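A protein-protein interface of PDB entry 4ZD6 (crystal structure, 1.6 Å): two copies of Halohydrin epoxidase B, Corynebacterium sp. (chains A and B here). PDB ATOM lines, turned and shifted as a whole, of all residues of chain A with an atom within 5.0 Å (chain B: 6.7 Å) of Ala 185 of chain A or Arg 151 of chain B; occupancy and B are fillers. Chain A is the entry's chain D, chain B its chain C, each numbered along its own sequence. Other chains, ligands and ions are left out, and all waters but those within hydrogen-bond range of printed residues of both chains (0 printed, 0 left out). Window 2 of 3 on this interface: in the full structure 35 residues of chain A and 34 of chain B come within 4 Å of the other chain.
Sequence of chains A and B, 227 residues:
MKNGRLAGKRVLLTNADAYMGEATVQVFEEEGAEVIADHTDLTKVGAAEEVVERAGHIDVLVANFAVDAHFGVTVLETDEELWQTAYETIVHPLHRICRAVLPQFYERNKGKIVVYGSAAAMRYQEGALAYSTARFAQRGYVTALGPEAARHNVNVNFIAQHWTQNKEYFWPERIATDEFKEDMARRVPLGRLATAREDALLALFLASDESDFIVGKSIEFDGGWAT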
ATOM      1  N   PHE A 180     -12.918  17.173 -11.916  1.00  0.00           N
ATOM      2  CA  PHE A 180     -13.722  17.077 -13.135  1.00  0.00           C
ATOM      3  C   PHE A 180     -14.004  18.449 -13.737  1.00  0.00           C
ATOM      4  O   PHE A 180     -13.929  18.615 -14.959  1.00  0.00           O
ATOM      5  CB  PHE A 180     -15.042  16.352 -12.868  1.00  0.00           C
ATOM      6  CG  PHE A 180     -15.903  16.207 -14.100  1.00  0.00           C
ATOM      7  CD1 PHE A 180     -15.781  15.097 -14.914  1.00  0.00           C
ATOM      8  CD2 PHE A 180     -16.819  17.194 -14.453  1.00  0.00           C
ATOM      9  CE1 PHE A 180     -16.557  14.966 -16.052  1.00  0.00           C
ATOM     10  CE2 PHE A 180     -17.595  17.070 -15.588  1.00  0.00           C
ATOM     11  CZ  PHE A 180     -17.459  15.959 -16.391  1.00  0.00           C
ATOM     12  N   LYS A 181     -14.360  19.433 -12.906  1.00  0.00           N
ATOM     13  CA  LYS A 181     -14.774  20.731 -13.436  1.00  0.00           C
ATOM     14  C   LYS A 181     -13.633  21.444 -14.155  1.00  0.00           C
ATOM     15  O   LYS A 181     -13.839  22.026 -15.225  1.00  0.00           O
ATOM     16  CB  LYS A 181     -15.333  21.605 -12.315  1.00  0.00           C
ATOM     17  CG  LYS A 181     -16.608  21.064 -11.699  1.00  0.00           C
ATOM     18  CD  LYS A 181     -16.924  21.743 -10.376  1.00  0.00           C
ATOM     19  CE  LYS A 181     -15.755  21.632  -9.410  1.00  0.00           C
ATOM     20  NZ  LYS A 181     -16.050  20.701  -8.286  1.00  0.00           N
ATOM     21  N   GLU A 182     -12.424  21.419 -13.593  1.00  0.00           N
ATOM     22  CA  GLU A 182     -11.317  22.057 -14.294  1.00  0.00           C
ATOM     23  C   GLU A 182     -10.706  21.144 -15.349  1.00  0.00           C
ATOM     24  O   GLU A 182     -10.097  21.637 -16.307  1.00  0.00           O
ATOM     25  CB  GLU A 182     -10.262  22.544 -13.301  1.00  0.00           C
ATOM     26  CG  GLU A 182     -10.846  23.382 -12.174  1.00  0.00           C
ATOM     27  CD  GLU A 182     -11.426  24.690 -12.681  1.00  0.00           C
ATOM     28  OE1 GLU A 182     -10.678  25.476 -13.308  1.00  0.00           O
ATOM     29  OE2 GLU A 182     -12.639  24.922 -12.465  1.00  0.00           O
ATOM     30  N   ASP A 183     -10.875  19.827 -15.220  1.00  0.00           N
ATOM     31  CA  ASP A 183     -10.625  18.948 -16.355  1.00  0.00           C
ATOM     32  C   ASP A 183     -11.427  19.405 -17.569  1.00  0.00           C
ATOM     33  O   ASP A 183     -10.878  19.606 -18.660  1.00  0.00           O
ATOM     34  CB  ASP A 183     -10.996  17.516 -15.981  1.00  0.00           C
ATOM     35  CG  ASP A 183     -10.159  16.485 -16.689  1.00  0.00           C
ATOM     36  OD1 ASP A 183      -9.124  16.062 -16.121  1.00  0.00           O
ATOM     37  OD2 ASP A 183     -10.557  16.070 -17.799  1.00  0.00           O
ATOM     38  N   MET A 184     -12.739  19.576 -17.385  1.00  0.00           N
ATOM     39  CA  MET A 184     -13.621  19.986 -18.474  1.00  0.00           C
ATOM     40  C   MET A 184     -13.268  21.385 -18.969  1.00  0.00           C
ATOM     41  O   MET A 184     -13.209  21.633 -20.179  1.00  0.00           O
ATOM     42  CB  MET A 184     -15.075  19.928 -17.991  1.00  0.00           C
ATOM     43  CG  MET A 184     -16.080  20.742 -18.804  1.00  0.00           C
ATOM     44  SD  MET A 184     -17.766  20.166 -18.538  1.00  0.00           S
ATOM     45  CE  MET A 184     -18.346  21.375 -17.371  1.00  0.00           C
ATOM     46  N   ALA A 185     -13.026  22.316 -18.043  1.00  0.00           N
ATOM     47  CA  ALA A 185     -12.673  23.675 -18.441  1.00  0.00           C
ATOM     48  C   ALA A 185     -11.380  23.698 -19.244  1.00  0.00           C
ATOM     49  O   ALA A 185     -11.240  24.475 -20.193  1.00  0.00           O
ATOM     50  CB  ALA A 185     -12.552  24.570 -17.207  1.00  0.00           C
ATOM     51  N   ARG A 186     -10.422  22.848 -18.883  1.00  0.00           N
ATOM     52  CA  ARG A 186      -9.148  22.844 -19.595  1.00  0.00           C
ATOM     53  C   ARG A 186      -9.284  22.224 -20.980  1.00  0.00           C
ATOM     54  O   ARG A 186      -8.639  22.683 -21.930  1.00  0.00           O
ATOM     55  CB  ARG A 186      -8.101  22.090 -18.772  1.00  0.00           C
ATOM     56  CG  ARG A 186      -6.676  22.155 -19.321  1.00  0.00           C
ATOM     57  CD  ARG A 186      -5.778  21.037 -18.756  1.00  0.00           C
ATOM     58  NE  ARG A 186      -5.868  20.917 -17.300  1.00  0.00           N
ATOM     59  CZ  ARG A 186      -6.460  19.910 -16.662  1.00  0.00           C
ATOM     60  NH1 ARG A 186      -7.017  18.921 -17.347  1.00  0.00           N
ATOM     61  NH2 ARG A 186      -6.500  19.889 -15.336  1.00  0.00           N
ATOM     62  N   ARG A 187     -10.134  21.210 -21.125  1.00  0.00           N
ATOM     63  CA  ARG A 187     -10.094  20.363 -22.307  1.00  0.00           C
ATOM     64  C   ARG A 187     -11.353  20.392 -23.166  1.00  0.00           C
ATOM     65  O   ARG A 187     -11.332  19.817 -24.265  1.00  0.00           O
ATOM     66  CB  ARG A 187      -9.801  18.908 -21.902  1.00  0.00           C
ATOM     67  CG  ARG A 187      -8.399  18.691 -21.313  1.00  0.00           C
ATOM     68  CD  ARG A 187      -7.280  19.081 -22.287  1.00  0.00           C
ATOM     69  NE  ARG A 187      -7.279  18.257 -23.497  1.00  0.00           N
ATOM     70  CZ  ARG A 187      -6.665  17.082 -23.586  1.00  0.00           C
ATOM     71  NH1 ARG A 187      -6.004  16.601 -22.535  1.00  0.00           N
ATOM     72  NH2 ARG A 187      -6.716  16.387 -24.715  1.00  0.00           N
ATOM     73  N   VAL A 188     -12.430  21.039 -22.725  1.00  0.00           N
ATOM     74  CA  VAL A 188     -13.642  21.164 -23.540  1.00  0.00           C
ATOM     75  C   VAL A 188     -13.819  22.630 -23.910  1.00  0.00           C
ATOM     76  O   VAL A 188     -14.245  23.439 -23.066  1.00  0.00           O
ATOM     77  CB  VAL A 188     -14.889  20.624 -22.816  1.00  0.00           C
ATOM     78  CG1 VAL A 188     -16.098  20.662 -23.754  1.00  0.00           C
ATOM     79  CG2 VAL A 188     -14.648  19.202 -22.326  1.00  0.00           C
ATOM     80  N   PRO A 189     -13.497  23.017 -25.150  1.00  0.00           N
ATOM     81  CA  PRO A 189     -13.595  24.432 -25.526  1.00  0.00           C
ATOM     82  C   PRO A 189     -14.945  25.052 -25.214  1.00  0.00           C
ATOM     83  O   PRO A 189     -15.001  26.185 -24.725  1.00  0.00           O
ATOM     84  CB  PRO A 189     -13.303  24.405 -27.037  1.00  0.00           C
ATOM     85  CG  PRO A 189     -12.380  23.241 -27.208  1.00  0.00           C
ATOM     86  CD  PRO A 189     -12.857  22.198 -26.199  1.00  0.00           C
ATOM     87  N   GLY A 191     -16.880  24.312 -22.825  1.00  0.00           N
ATOM     88  CA  GLY A 191     -16.942  24.551 -21.392  1.00  0.00           C
ATOM     89  C   GLY A 191     -18.112  23.933 -20.667  1.00  0.00           C
ATOM     90  O   GLY A 191     -18.383  24.307 -19.520  1.00  0.00           O
ATOM     91  N   TYR B 106     -19.653  37.975 -29.843  1.00  0.00           N
ATOM     92  CA  TYR B 106     -19.002  37.992 -28.542  1.00  0.00           C
ATOM     93  C   TYR B 106     -19.789  38.819 -27.538  1.00  0.00           C
ATOM     94  O   TYR B 106     -19.813  38.488 -26.346  1.00  0.00           O
ATOM     95  CB  TYR B 106     -17.578  38.527 -28.683  1.00  0.00           C
ATOM     96  CG  TYR B 106     -16.596  37.543 -29.300  1.00  0.00           C
ATOM     97  CD1 TYR B 106     -16.974  36.241 -29.628  1.00  0.00           C
ATOM     98  CD2 TYR B 106     -15.282  37.920 -29.541  1.00  0.00           C
ATOM     99  CE1 TYR B 106     -16.058  35.345 -30.182  1.00  0.00           C
ATOM    100  CE2 TYR B 106     -14.368  37.040 -30.096  1.00  0.00           C
ATOM    101  CZ  TYR B 106     -14.752  35.758 -30.409  1.00  0.00           C
ATOM    102  OH  TYR B 106     -13.807  34.904 -30.950  1.00  0.00           O
ATOM    103  N   ASN B 109     -22.509  36.392 -26.556  1.00  0.00           N
ATOM    104  CA  ASN B 109     -22.068  35.052 -26.186  1.00  0.00           C
ATOM    105  C   ASN B 109     -22.873  33.993 -26.937  1.00  0.00           C
ATOM    106  O   ASN B 109     -23.380  33.040 -26.350  1.00  0.00           O
ATOM    107  CB  ASN B 109     -22.169  34.842 -24.680  1.00  0.00           C
ATOM    108  CG  ASN B 109     -21.148  33.861 -24.163  1.00  0.00           C
ATOM    109  OD1 ASN B 109     -21.494  32.781 -23.681  1.00  0.00           O
ATOM    110  ND2 ASN B 109     -19.872  34.227 -24.272  1.00  0.00           N
ATOM    111  N   GLY B 146     -12.394  27.494 -34.344  1.00  0.00           N
ATOM    112  CA  GLY B 146     -13.463  26.797 -33.659  1.00  0.00           C
ATOM    113  C   GLY B 146     -13.360  26.808 -32.145  1.00  0.00           C
ATOM    114  O   GLY B 146     -14.269  27.268 -31.453  1.00  0.00           O
ATOM    115  N   PRO B 147     -12.264  26.288 -31.596  1.00  0.00           N
ATOM    116  CA  PRO B 147     -12.163  26.219 -30.129  1.00  0.00           C
ATOM    117  C   PRO B 147     -12.010  27.585 -29.483  1.00  0.00           C
ATOM    118  O   PRO B 147     -12.487  27.779 -28.358  1.00  0.00           O
ATOM    119  CB  PRO B 147     -10.931  25.332 -29.907  1.00  0.00           C
ATOM    120  CG  PRO B 147     -10.819  24.523 -31.175  1.00  0.00           C
ATOM    121  CD  PRO B 147     -11.214  25.488 -32.251  1.00  0.00           C
ATOM    122  N   GLU B 148     -11.389  28.545 -30.176  1.00  0.00           N
ATOM    123  CA  GLU B 148     -11.309  29.911 -29.653  1.00  0.00           C
ATOM    124  C   GLU B 148     -12.694  30.537 -29.529  1.00  0.00           C
ATOM    125  O   GLU B 148     -13.034  31.144 -28.500  1.00  0.00           O
ATOM    126  CB  GLU B 148     -10.419  30.756 -30.570  1.00  0.00           C
ATOM    127  CG  GLU B 148     -10.367  32.232 -30.209  1.00  0.00           C
ATOM    128  CD  GLU B 148      -9.396  33.040 -31.069  1.00  0.00           C
ATOM    129  OE1 GLU B 148      -8.679  32.451 -31.912  1.00  0.00           O
ATOM    130  OE2 GLU B 148      -9.343  34.278 -30.896  1.00  0.00           O
ATOM    131  N   ALA B 149     -13.501  30.424 -30.590  1.00  0.00           N
ATOM    132  CA  ALA B 149     -14.839  31.000 -30.588  1.00  0.00           C
ATOM    133  C   ALA B 149     -15.781  30.239 -29.664  1.00  0.00           C
ATOM    134  O   ALA B 149     -16.707  30.834 -29.097  1.00  0.00           O
ATOM    135  CB  ALA B 149     -15.379  31.031 -32.023  1.00  0.00           C
ATOM    136  N   ALA B 150     -15.556  28.937 -29.485  1.00  0.00           N
ATOM    137  CA  ALA B 150     -16.439  28.153 -28.626  1.00  0.00           C
ATOM    138  C   ALA B 150     -16.416  28.656 -27.194  1.00  0.00           C
ATOM    139  O   ALA B 150     -17.375  28.439 -26.447  1.00  0.00           O
ATOM    140  CB  ALA B 150     -16.045  26.677 -28.652  1.00  0.00           C
ATOM    141  N   ARG B 151     -15.309  29.277 -26.783  1.00  0.00           N
ATOM    142  CA  ARG B 151     -15.226  29.878 -25.462  1.00  0.00           C
ATOM    143  C   ARG B 151     -16.276  30.961 -25.272  1.00  0.00           C
ATOM    144  O   ARG B 151     -16.666  31.234 -24.130  1.00  0.00           O
ATOM    145  CB  ARG B 151     -13.811  30.446 -25.245  1.00  0.00           C
ATOM    146  CG  ARG B 151     -12.730  29.387 -25.116  1.00  0.00           C
ATOM    147  CD  ARG B 151     -13.070  28.485 -23.917  1.00  0.00           C
ATOM    148  NE  ARG B 151     -12.101  27.411 -23.788  1.00  0.00           N
ATOM    149  CZ  ARG B 151     -12.127  26.513 -22.803  1.00  0.00           C
ATOM    150  NH1 ARG B 151     -13.073  26.559 -21.855  1.00  0.00           N
ATOM    151  NH2 ARG B 151     -11.198  25.559 -22.754  1.00  0.00           N
ATOM    152  N   HIS B 152     -16.763  31.542 -26.370  1.00  0.00           N
ATOM    153  CA  HIS B 152     -17.843  32.516 -26.386  1.00  0.00           C
ATOM    154  C   HIS B 152     -19.160  31.906 -26.864  1.00  0.00           C
ATOM    155  O   HIS B 152     -20.050  32.643 -27.298  1.00  0.00           O
ATOM    156  CB  HIS B 152     -17.465  33.705 -27.276  1.00  0.00           C
ATOM    157  CG  HIS B 152     -16.263  34.462 -26.807  1.00  0.00           C
ATOM    158  ND1 HIS B 152     -16.355  35.564 -25.984  1.00  0.00           N
ATOM    159  CD2 HIS B 152     -14.939  34.271 -27.033  1.00  0.00           C
ATOM    160  CE1 HIS B 152     -15.142  36.024 -25.730  1.00  0.00           C
ATOM    161  NE2 HIS B 152     -14.266  35.259 -26.357  1.00  0.00           N
ATOM    162  N   ASN B 153     -19.287  30.576 -26.823  1.00  0.00           N
ATOM    163  CA  ASN B 153     -20.509  29.884 -27.239  1.00  0.00           C
ATOM    164  C   ASN B 153     -20.824  30.139 -28.719  1.00  0.00           C
ATOM    165  O   ASN B 153     -21.988  30.218 -29.115  1.00  0.00           O
ATOM    166  CB  ASN B 153     -21.689  30.290 -26.338  1.00  0.00           C
ATOM    167  CG  ASN B 153     -22.895  29.347 -26.442  1.00  0.00           C
ATOM    168  OD1 ASN B 153     -22.760  28.122 -26.558  1.00  0.00           O
ATOM    169  ND2 ASN B 153     -24.090  29.929 -26.376  1.00  0.00           N
ATOM    170  N   VAL B 154     -19.787  30.285 -29.544  1.00  0.00           N
ATOM    171  CA  VAL B 154     -19.925  30.450 -30.986  1.00  0.00           C
ATOM    172  C   VAL B 154     -19.459  29.166 -31.652  1.00  0.00           C
ATOM    173  O   VAL B 154     -18.354  28.683 -31.361  1.00  0.00           O
ATOM    174  CB  VAL B 154     -19.111  31.646 -31.508  1.00  0.00           C
ATOM    175  CG1 VAL B 154     -19.157  31.694 -33.030  1.00  0.00           C
ATOM    176  CG2 VAL B 154     -19.605  32.959 -30.902  1.00  0.00           C
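The guanidinium group (NH2) of Arg 151 of chain B lies within hydrogen-bond range of the backbone carbonyl oxygen (O) of Ala 185 of chain A, 2.8 Å away.
NE of Arg 151 of chain B lies close to O of Pro 189 of chain A (3.3 Å).
OD1 of Asp 183 of chain A is in salt-bridge range of NH1 of Arg 186 of chain A, 3.8 Å away.
Arg 186 of chain A touches Arg 151 of chain B (O to NH2, 3.9 Å).
Arg 151 of chain B touches Val 188 of chain A (NH1 to O, 3.5 Å).
Pro 189 of chain A touches Pro 147 of chain B (CG to CB, 3.7 Å).
Ala 150 of chain B touches Pro 189 of chain A (O to O, 3.7 Å).
Of chain B, only Arg 151 comes within 4 Å of Ala 185 of chain A.
Arg 151 of chain B touches just these residues of chain A: Ala 185, Arg 186, Val 188 and Pro 189.
Of the printed residues of chain A, Ala 150 of chain B touches Pro 189 (3.7 Å).
Of the printed residues of chain B, Pro 189 of chain A touches Pro 147 (3.7 Å), Ala 150 (3.7 Å) and Arg 151 (3.1 Å).
Of the printed residues of chain A, Pro 147 of chain B touches Pro 189.
Printed residues of chain B within 4 Å of Arg 186 of chain A: Arg 151 (3.9 Å).
Of the printed residues of chain B, Val 188 of chain A touches Arg 151 (3.5 Å).
Phe 180 of chain A touches none of the printed residues of chain B.
The nearest printed residue of chain A that does not touch Pro 147 of chain B is Val 188 of chain A (6.9 Å).
Of the 11 printed residues of chain B, 3 touch a printed residue of chain A.
Along chain B the printed residues that touch a printed residue of chain A span positions 147 to 151.
Of the 11 printed residues of chain A, 4 touch a printed residue of chain B.
Hydrophobic or aromatic side chains of chain A within 4 Å of the printed part of chain B: Pro 189.
Among the printed residues, 6 pairs touch across the chains.
No position is printed for both chains.
Of the 6 pairs that touch across the chains among the printed residues, none has its exchanged pair printed and touching as well.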
